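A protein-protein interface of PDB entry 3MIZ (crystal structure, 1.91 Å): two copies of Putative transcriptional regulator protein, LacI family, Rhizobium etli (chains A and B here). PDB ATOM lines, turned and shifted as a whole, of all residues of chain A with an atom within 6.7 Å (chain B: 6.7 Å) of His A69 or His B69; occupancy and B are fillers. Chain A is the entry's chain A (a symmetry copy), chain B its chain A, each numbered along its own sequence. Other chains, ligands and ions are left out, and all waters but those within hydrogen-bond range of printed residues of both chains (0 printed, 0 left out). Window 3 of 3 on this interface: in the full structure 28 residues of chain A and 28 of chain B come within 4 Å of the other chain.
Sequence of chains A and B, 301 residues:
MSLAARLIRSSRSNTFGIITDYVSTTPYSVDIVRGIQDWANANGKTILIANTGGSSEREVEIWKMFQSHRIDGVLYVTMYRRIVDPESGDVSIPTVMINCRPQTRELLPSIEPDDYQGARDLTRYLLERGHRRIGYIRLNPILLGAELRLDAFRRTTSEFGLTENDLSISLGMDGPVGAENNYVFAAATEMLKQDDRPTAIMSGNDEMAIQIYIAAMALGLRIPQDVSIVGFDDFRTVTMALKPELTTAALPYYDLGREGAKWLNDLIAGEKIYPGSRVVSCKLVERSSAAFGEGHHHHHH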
ATOM      1  N   SER A  13      20.959 -13.679  -2.596  1.00  0.00           N
ATOM      2  CA  SER A  13      20.565 -13.083  -1.326  1.00  0.00           C
ATOM      3  C   SER A  13      20.360 -11.584  -1.507  1.00  0.00           C
ATOM      4  O   SER A  13      19.704 -10.933  -0.690  1.00  0.00           O
ATOM      5  CB  SER A  13      21.644 -13.320  -0.268  1.00  0.00           C
ATOM      6  OG  SER A  13      22.836 -12.632  -0.603  1.00  0.00           O
ATOM      7  N   THR A  15      22.637  -9.543  -1.291  1.00  0.00           N
ATOM      8  CA  THR A  15      23.484  -8.947  -0.269  1.00  0.00           C
ATOM      9  C   THR A  15      24.927  -8.897  -0.756  1.00  0.00           C
ATOM     10  O   THR A  15      25.478  -9.907  -1.198  1.00  0.00           O
ATOM     11  CB  THR A  15      23.421  -9.762   1.044  1.00  0.00           C
ATOM     12  OG1 THR A  15      22.067  -9.798   1.513  1.00  0.00           O
ATOM     13  CG2 THR A  15      24.303  -9.132   2.113  1.00  0.00           C
ATOM     14  N   LEU A  48      26.738  -5.623   3.933  1.00  0.00           N
ATOM     15  CA  LEU A  48      27.296  -6.061   5.207  1.00  0.00           C
ATOM     16  C   LEU A  48      28.787  -5.770   5.136  1.00  0.00           C
ATOM     17  O   LEU A  48      29.454  -6.151   4.170  1.00  0.00           O
ATOM     18  CB  LEU A  48      27.082  -7.558   5.423  1.00  0.00           C
ATOM     19  CG  LEU A  48      25.702  -7.997   5.919  1.00  0.00           C
ATOM     20  CD1 LEU A  48      25.653  -9.526   6.033  1.00  0.00           C
ATOM     21  CD2 LEU A  48      25.432  -7.351   7.275  1.00  0.00           C
ATOM     22  N   LYS A  64      35.544 -16.875   4.542  1.00  0.00           N
ATOM     23  CA  LYS A  64      34.865 -18.113   4.897  1.00  0.00           C
ATOM     24  C   LYS A  64      33.479 -17.756   5.434  1.00  0.00           C
ATOM     25  O   LYS A  64      32.482 -18.380   5.075  1.00  0.00           O
ATOM     26  CB  LYS A  64      35.681 -18.852   5.961  1.00  0.00           C
ATOM     27  CG  LYS A  64      35.576 -20.358   5.906  1.00  0.00           C
ATOM     28  CD  LYS A  64      36.647 -21.016   6.770  1.00  0.00           C
ATOM     29  CE  LYS A  64      38.061 -20.662   6.303  1.00  0.00           C
ATOM     30  NZ  LYS A  64      38.330 -21.104   4.904  1.00  0.00           N
ATOM     31  N   MET A  65      33.426 -16.745   6.293  1.00  0.00           N
ATOM     32  CA  MET A  65      32.160 -16.293   6.860  1.00  0.00           C
ATOM     33  C   MET A  65      31.195 -15.841   5.769  1.00  0.00           C
ATOM     34  O   MET A  65      30.010 -16.180   5.799  1.00  0.00           O
ATOM     35  CB  MET A  65      32.388 -15.138   7.840  1.00  0.00           C
ATOM     36  CG  MET A  65      31.125 -14.325   8.143  1.00  0.00           C
ATOM     37  SD  MET A  65      31.354 -13.156   9.657  1.00  0.00           S
ATOM     38  CE  MET A  65      31.194 -14.516  11.019  1.00  0.00           C
ATOM     39  N   PHE A  66      31.692 -15.066   4.810  1.00  0.00           N
ATOM     40  CA  PHE A  66      30.829 -14.591   3.736  1.00  0.00           C
ATOM     41  C   PHE A  66      30.282 -15.725   2.880  1.00  0.00           C
ATOM     42  O   PHE A  66      29.124 -15.687   2.464  1.00  0.00           O
ATOM     43  CB  PHE A  66      31.551 -13.561   2.860  1.00  0.00           C
ATOM     44  CG  PHE A  66      31.538 -12.166   3.431  1.00  0.00           C
ATOM     45  CD1 PHE A  66      30.469 -11.733   4.213  1.00  0.00           C
ATOM     46  CD2 PHE A  66      32.573 -11.277   3.169  1.00  0.00           C
ATOM     47  CE1 PHE A  66      30.430 -10.434   4.725  1.00  0.00           C
ATOM     48  CE2 PHE A  66      32.539  -9.973   3.678  1.00  0.00           C
ATOM     49  CZ  PHE A  66      31.471  -9.554   4.454  1.00  0.00           C
ATOM     50  N   GLN A  67      31.104 -16.733   2.614  1.00  0.00           N
ATOM     51  CA  GLN A  67      30.643 -17.862   1.819  1.00  0.00           C
ATOM     52  C   GLN A  67      29.509 -18.531   2.586  1.00  0.00           C
ATOM     53  O   GLN A  67      28.453 -18.815   2.028  1.00  0.00           O
ATOM     54  CB  GLN A  67      31.770 -18.872   1.585  1.00  0.00           C
ATOM     55  CG  GLN A  67      31.350 -20.056   0.708  1.00  0.00           C
ATOM     56  CD  GLN A  67      32.487 -21.024   0.443  1.00  0.00           C
ATOM     57  OE1 GLN A  67      33.022 -21.637   1.366  1.00  0.00           O
ATOM     58  NE2 GLN A  67      32.865 -21.163  -0.824  1.00  0.00           N
ATOM     59  N   SER A  68      29.743 -18.757   3.874  1.00  0.00           N
ATOM     60  CA  SER A  68      28.761 -19.381   4.754  1.00  0.00           C
ATOM     61  C   SER A  68      27.416 -18.651   4.747  1.00  0.00           C
ATOM     62  O   SER A  68      26.361 -19.280   4.793  1.00  0.00           O
ATOM     63  CB  SER A  68      29.304 -19.419   6.187  1.00  0.00           C
ATOM     64  OG  SER A  68      28.297 -19.792   7.109  1.00  0.00           O
ATOM     65  N   HIS A  69      27.467 -17.323   4.685  1.00  0.00           N
ATOM     66  CA  HIS A  69      26.264 -16.494   4.691  1.00  0.00           C
ATOM     67  C   HIS A  69      25.633 -16.269   3.314  1.00  0.00           C
ATOM     68  O   HIS A  69      24.663 -15.518   3.187  1.00  0.00           O
ATOM     69  CB  HIS A  69      26.582 -15.147   5.347  1.00  0.00           C
ATOM     70  CG  HIS A  69      26.725 -15.219   6.836  1.00  0.00           C
ATOM     71  ND1 HIS A  69      25.643 -15.344   7.683  1.00  0.00           N
ATOM     72  CD2 HIS A  69      27.820 -15.179   7.632  1.00  0.00           C
ATOM     73  CE1 HIS A  69      26.066 -15.375   8.935  1.00  0.00           C
ATOM     74  NE2 HIS A  69      27.383 -15.276   8.930  1.00  0.00           N
ATOM     75  N   ARG A  70      26.185 -16.921   2.294  1.00  0.00           N
ATOM     76  CA  ARG A  70      25.687 -16.824   0.918  1.00  0.00           C
ATOM     77  C   ARG A  70      25.700 -15.422   0.306  1.00  0.00           C
ATOM     78  O   ARG A  70      24.801 -15.062  -0.453  1.00  0.00           O
ATOM     79  CB  ARG A  70      24.266 -17.391   0.817  1.00  0.00           C
ATOM     80  CG  ARG A  70      24.042 -18.702   1.566  1.00  0.00           C
ATOM     81  CD  ARG A  70      25.069 -19.763   1.211  1.00  0.00           C
ATOM     82  NE  ARG A  70      24.867 -20.976   2.001  1.00  0.00           N
ATOM     83  CZ  ARG A  70      25.750 -21.967   2.092  1.00  0.00           C
ATOM     84  NH1 ARG A  70      26.905 -21.894   1.443  1.00  0.00           N
ATOM     85  NH2 ARG A  70      25.476 -23.034   2.835  1.00  0.00           N
ATOM     86  N   ILE A  71      26.705 -14.623   0.642  1.00  0.00           N
ATOM     87  CA  ILE A  71      26.817 -13.284   0.068  1.00  0.00           C
ATOM     88  C   ILE A  71      26.926 -13.446  -1.453  1.00  0.00           C
ATOM     89  O   ILE A  71      27.589 -14.365  -1.932  1.00  0.00           O
ATOM     90  CB  ILE A  71      28.076 -12.562   0.595  1.00  0.00           C
ATOM     91  CG1 ILE A  71      27.937 -12.314   2.100  1.00  0.00           C
ATOM     92  CG2 ILE A  71      28.281 -11.252  -0.145  1.00  0.00           C
ATOM     93  CD1 ILE A  71      26.721 -11.477   2.474  1.00  0.00           C
ATOM     94  N   ASP A  72      26.268 -12.565  -2.204  1.00  0.00           N
ATOM     95  CA  ASP A  72      26.291 -12.632  -3.665  1.00  0.00           C
ATOM     96  C   ASP A  72      27.603 -12.158  -4.284  1.00  0.00           C
ATOM     97  O   ASP A  72      28.022 -12.666  -5.323  1.00  0.00           O
ATOM     98  CB  ASP A  72      25.148 -11.812  -4.269  1.00  0.00           C
ATOM     99  CG  ASP A  72      23.792 -12.439  -4.037  1.00  0.00           C
ATOM    100  OD1 ASP A  72      23.734 -13.657  -3.759  1.00  0.00           O
ATOM    101  OD2 ASP A  72      22.782 -11.707  -4.149  1.00  0.00           O
ATOM    102  N   SER B  13      27.128 -18.458  16.775  1.00  0.00           N
ATOM    103  CA  SER B  13      27.929 -18.182  15.591  1.00  0.00           C
ATOM    104  C   SER B  13      29.189 -17.424  15.994  1.00  0.00           C
ATOM    105  O   SER B  13      30.168 -17.383  15.245  1.00  0.00           O
ATOM    106  CB  SER B  13      27.133 -17.340  14.592  1.00  0.00           C
ATOM    107  OG  SER B  13      26.863 -16.054  15.121  1.00  0.00           O
ATOM    108  N   THR B  15      29.291 -14.373  16.276  1.00  0.00           N
ATOM    109  CA  THR B  15      29.276 -13.191  15.427  1.00  0.00           C
ATOM    110  C   THR B  15      28.349 -12.139  16.023  1.00  0.00           C
ATOM    111  O   THR B  15      27.191 -12.425  16.338  1.00  0.00           O
ATOM    112  CB  THR B  15      28.794 -13.542  14.001  1.00  0.00           C
ATOM    113  OG1 THR B  15      29.674 -14.520  13.432  1.00  0.00           O
ATOM    114  CG2 THR B  15      28.785 -12.304  13.114  1.00  0.00           C
ATOM    115  N   LEU B  48      30.023  -7.955  12.064  1.00  0.00           N
ATOM    116  CA  LEU B  48      29.425  -7.602  10.782  1.00  0.00           C
ATOM    117  C   LEU B  48      28.680  -6.295  11.009  1.00  0.00           C
ATOM    118  O   LEU B  48      27.889  -6.182  11.949  1.00  0.00           O
ATOM    119  CB  LEU B  48      28.440  -8.671  10.314  1.00  0.00           C
ATOM    120  CG  LEU B  48      29.031  -9.918   9.653  1.00  0.00           C
ATOM    121  CD1 LEU B  48      27.908 -10.899   9.293  1.00  0.00           C
ATOM    122  CD2 LEU B  48      29.798  -9.501   8.401  1.00  0.00           C
ATOM    123  N   LYS B  64      15.830  -8.228  10.327  1.00  0.00           N
ATOM    124  CA  LYS B  64      15.351  -9.466   9.730  1.00  0.00           C
ATOM    125  C   LYS B  64      16.556 -10.211   9.155  1.00  0.00           C
ATOM    126  O   LYS B  64      16.697 -11.420   9.334  1.00  0.00           O
ATOM    127  CB  LYS B  64      14.343  -9.141   8.624  1.00  0.00           C
ATOM    128  CG  LYS B  64      13.260 -10.176   8.431  1.00  0.00           C
ATOM    129  CD  LYS B  64      12.134  -9.636   7.555  1.00  0.00           C
ATOM    130  CE  LYS B  64      11.458  -8.412   8.176  1.00  0.00           C
ATOM    131  NZ  LYS B  64      10.843  -8.708   9.504  1.00  0.00           N
ATOM    132  N   MET B  65      17.424  -9.479   8.466  1.00  0.00           N
ATOM    133  CA  MET B  65      18.627 -10.069   7.885  1.00  0.00           C
ATOM    134  C   MET B  65      19.511 -10.692   8.960  1.00  0.00           C
ATOM    135  O   MET B  65      20.018 -11.803   8.787  1.00  0.00           O
ATOM    136  CB  MET B  65      19.431  -9.012   7.122  1.00  0.00           C
ATOM    137  CG  MET B  65      20.886  -9.414   6.859  1.00  0.00           C
ATOM    138  SD  MET B  65      21.741  -8.264   5.572  1.00  0.00           S
ATOM    139  CE  MET B  65      20.911  -9.023   4.003  1.00  0.00           C
ATOM    140  N   PHE B  66      19.708  -9.980  10.065  1.00  0.00           N
ATOM    141  CA  PHE B  66      20.547 -10.509  11.133  1.00  0.00           C
ATOM    142  C   PHE B  66      19.972 -11.776  11.754  1.00  0.00           C
ATOM    143  O   PHE B  66      20.716 -12.699  12.082  1.00  0.00           O
ATOM    144  CB  PHE B  66      20.799  -9.452  12.214  1.00  0.00           C
ATOM    145  CG  PHE B  66      21.912  -8.494  11.873  1.00  0.00           C
ATOM    146  CD1 PHE B  66      22.988  -8.911  11.093  1.00  0.00           C
ATOM    147  CD2 PHE B  66      21.904  -7.189  12.349  1.00  0.00           C
ATOM    148  CE1 PHE B  66      24.041  -8.042  10.793  1.00  0.00           C
ATOM    149  CE2 PHE B  66      22.955  -6.314  12.054  1.00  0.00           C
ATOM    150  CZ  PHE B  66      24.020  -6.740  11.276  1.00  0.00           C
ATOM    151  N   GLN B  67      18.655 -11.825  11.916  1.00  0.00           N
ATOM    152  CA  GLN B  67      18.033 -13.013  12.484  1.00  0.00           C
ATOM    153  C   GLN B  67      18.312 -14.174  11.538  1.00  0.00           C
ATOM    154  O   GLN B  67      18.735 -15.246  11.963  1.00  0.00           O
ATOM    155  CB  GLN B  67      16.521 -12.828  12.637  1.00  0.00           C
ATOM    156  CG  GLN B  67      15.825 -14.032  13.280  1.00  0.00           C
ATOM    157  CD  GLN B  67      14.336 -13.817  13.472  1.00  0.00           C
ATOM    158  OE1 GLN B  67      13.593 -13.648  12.506  1.00  0.00           O
ATOM    159  NE2 GLN B  67      13.892 -13.818  14.725  1.00  0.00           N
ATOM    160  N   SER B  68      18.086 -13.934  10.251  1.00  0.00           N
ATOM    161  CA  SER B  68      18.309 -14.933   9.212  1.00  0.00           C
ATOM    162  C   SER B  68      19.730 -15.498   9.236  1.00  0.00           C
ATOM    163  O   SER B  68      19.935 -16.690   9.011  1.00  0.00           O
ATOM    164  CB  SER B  68      18.036 -14.315   7.836  1.00  0.00           C
ATOM    165  OG  SER B  68      18.470 -15.168   6.794  1.00  0.00           O
ATOM    166  N   HIS B  69      20.703 -14.635   9.513  1.00  0.00           N
ATOM    167  CA  HIS B  69      22.110 -15.028   9.549  1.00  0.00           C
ATOM    168  C   HIS B  69      22.586 -15.587  10.893  1.00  0.00           C
ATOM    169  O   HIS B  69      23.772 -15.873  11.065  1.00  0.00           O
ATOM    170  CB  HIS B  69      22.979 -13.835   9.143  1.00  0.00           C
ATOM    171  CG  HIS B  69      22.944 -13.534   7.675  1.00  0.00           C
ATOM    172  ND1 HIS B  69      23.608 -14.300   6.741  1.00  0.00           N
ATOM    173  CD2 HIS B  69      22.328 -12.549   6.979  1.00  0.00           C
ATOM    174  CE1 HIS B  69      23.406 -13.799   5.536  1.00  0.00           C
ATOM    175  NE2 HIS B  69      22.632 -12.735   5.653  1.00  0.00           N
ATOM    176  N   ARG B  70      21.658 -15.739  11.834  1.00  0.00           N
ATOM    177  CA  ARG B  70      21.950 -16.277  13.167  1.00  0.00           C
ATOM    178  C   ARG B  70      22.963 -15.483  13.994  1.00  0.00           C
ATOM    179  O   ARG B  70      23.759 -16.062  14.731  1.00  0.00           O
ATOM    180  CB  ARG B  70      22.426 -17.731  13.071  1.00  0.00           C
ATOM    181  CG  ARG B  70      21.629 -18.606  12.107  1.00  0.00           C
ATOM    182  CD  ARG B  70      20.133 -18.548  12.364  1.00  0.00           C
ATOM    183  NE  ARG B  70      19.398 -19.338  11.378  1.00  0.00           N
ATOM    184  CZ  ARG B  70      18.081 -19.275  11.196  1.00  0.00           C
ATOM    185  NH1 ARG B  70      17.344 -18.453  11.933  1.00  0.00           N
ATOM    186  NH2 ARG B  70      17.501 -20.035  10.275  1.00  0.00           N
ATOM    187  N   ILE B  71      22.948 -14.162  13.867  1.00  0.00           N
ATOM    188  CA  ILE B  71      23.853 -13.327  14.653  1.00  0.00           C
ATOM    189  C   ILE B  71      23.546 -13.588  16.132  1.00  0.00           C
ATOM    190  O   ILE B  71      22.383 -13.738  16.506  1.00  0.00           O
ATOM    191  CB  ILE B  71      23.631 -11.831  14.342  1.00  0.00           C
ATOM    192  CG1 ILE B  71      24.021 -11.541  12.891  1.00  0.00           C
ATOM    193  CG2 ILE B  71      24.440 -10.969  15.296  1.00  0.00           C
ATOM    194  CD1 ILE B  71      25.469 -11.880  12.566  1.00  0.00           C
ATOM    195  N   ASP B  72      24.584 -13.654  16.964  1.00  0.00           N
ATOM    196  CA  ASP B  72      24.410 -13.912  18.393  1.00  0.00           C
ATOM    197  C   ASP B  72      23.879 -12.715  19.175  1.00  0.00           C
ATOM    198  O   ASP B  72      23.145 -12.880  20.149  1.00  0.00           O
ATOM    199  CB  ASP B  72      25.725 -14.363  19.033  1.00  0.00           C
ATOM    200  CG  ASP B  72      26.139 -15.753  18.602  1.00  0.00           C
ATOM    201  OD1 ASP B  72      25.269 -16.518  18.131  1.00  0.00           O
ATOM    202  OD2 ASP B  72      27.338 -16.079  18.754  1.00  0.00           O
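ND1 of His B69 lies within hydrogen-bond range of ND1 of His A69, 2.5 Å away.
OG of Ser B13 sits close to N of Thr B15. The backbone carbonyl oxygen (O) of Thr B15 sits at hydrogen-bond distance from the backbone NH (N) of Asp B72, 2.9 Å away. The backbone carbonyl oxygen of Phe B66 sits at hydrogen-bond distance from the backbone NH of Ile B71, at 3.2 Å. OG of Ser A13 sits close to N of Thr A15 (3.2 Å). The backbone carbonyl oxygen (O) of Thr A15 lies within hydrogen-bond range of the backbone NH (N) of Asp A72 (2.9 Å). O of Phe A66 sits at hydrogen-bond distance from N of Ile A71 (3.2 Å).
Among the printed residues, pairs that only touch across the chains: Met A65 with Thr B15 (2.9 Å), Thr A15 with Met B65 (2.9 Å), Phe A66 with Leu B48 (3.8 Å), Leu A48 with Phe B66 (3.8 Å), Met A65 with Leu B48 (3.99 Å) and Leu A48 with Met B65 (3.99 Å).
Ser A13 touches none of the printed residues of chain B. Of the printed residues of chain B, Thr A15 touches Met B65. Of the printed residues of chain B, Met A65 touches Thr B15 (2.9 Å) and Leu B48 (3.99 Å). Of the printed residues of chain B, Phe A66 touches Leu B48. His A69 touches one residue of chain B. Printed residues of chain A within 4 Å of Met B65: Thr A15 and Leu A48. Of chain A, only His A69 (2.5 Å) comes within 4 Å of His B69. Ile B71 touches none of the printed residues of chain A.
Of the 12 printed residues of chain B, 5 touch a printed residue of chain A. Hydrophobic or aromatic side chains of chain B within 4 Å of the printed part of chain A: Leu B48, Met B65, Phe B66 and His B69. Of the 12 printed residues of chain A, 5 touch a printed residue of chain B. Printed residues of chain A that touch a printed residue of chain B: Thr A15, Leu A48, Met A65, Phe A66 and His A69. Hydrophobic or aromatic side chains of chain A that line the printed part of chain B: Leu A48, Met A65, Phe A66 and His A69. Among the printed residues, 7 pairs touch across the chains. Among the printed residues, no Asp or Glu carboxylate lies within 4 Å of a Lys or Arg side-chain nitrogen of the other chain.
Thr A15 touches Met B65, and with the chains exchanged Met A65 touches Thr B15. Leu A48 touches Met B65, and with the chains exchanged Met A65 touches Leu B48. Leu A48 touches Phe B66, and with the chains exchanged Phe A66 touches Leu B48. His B69 touches its own counterpart, His A69.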
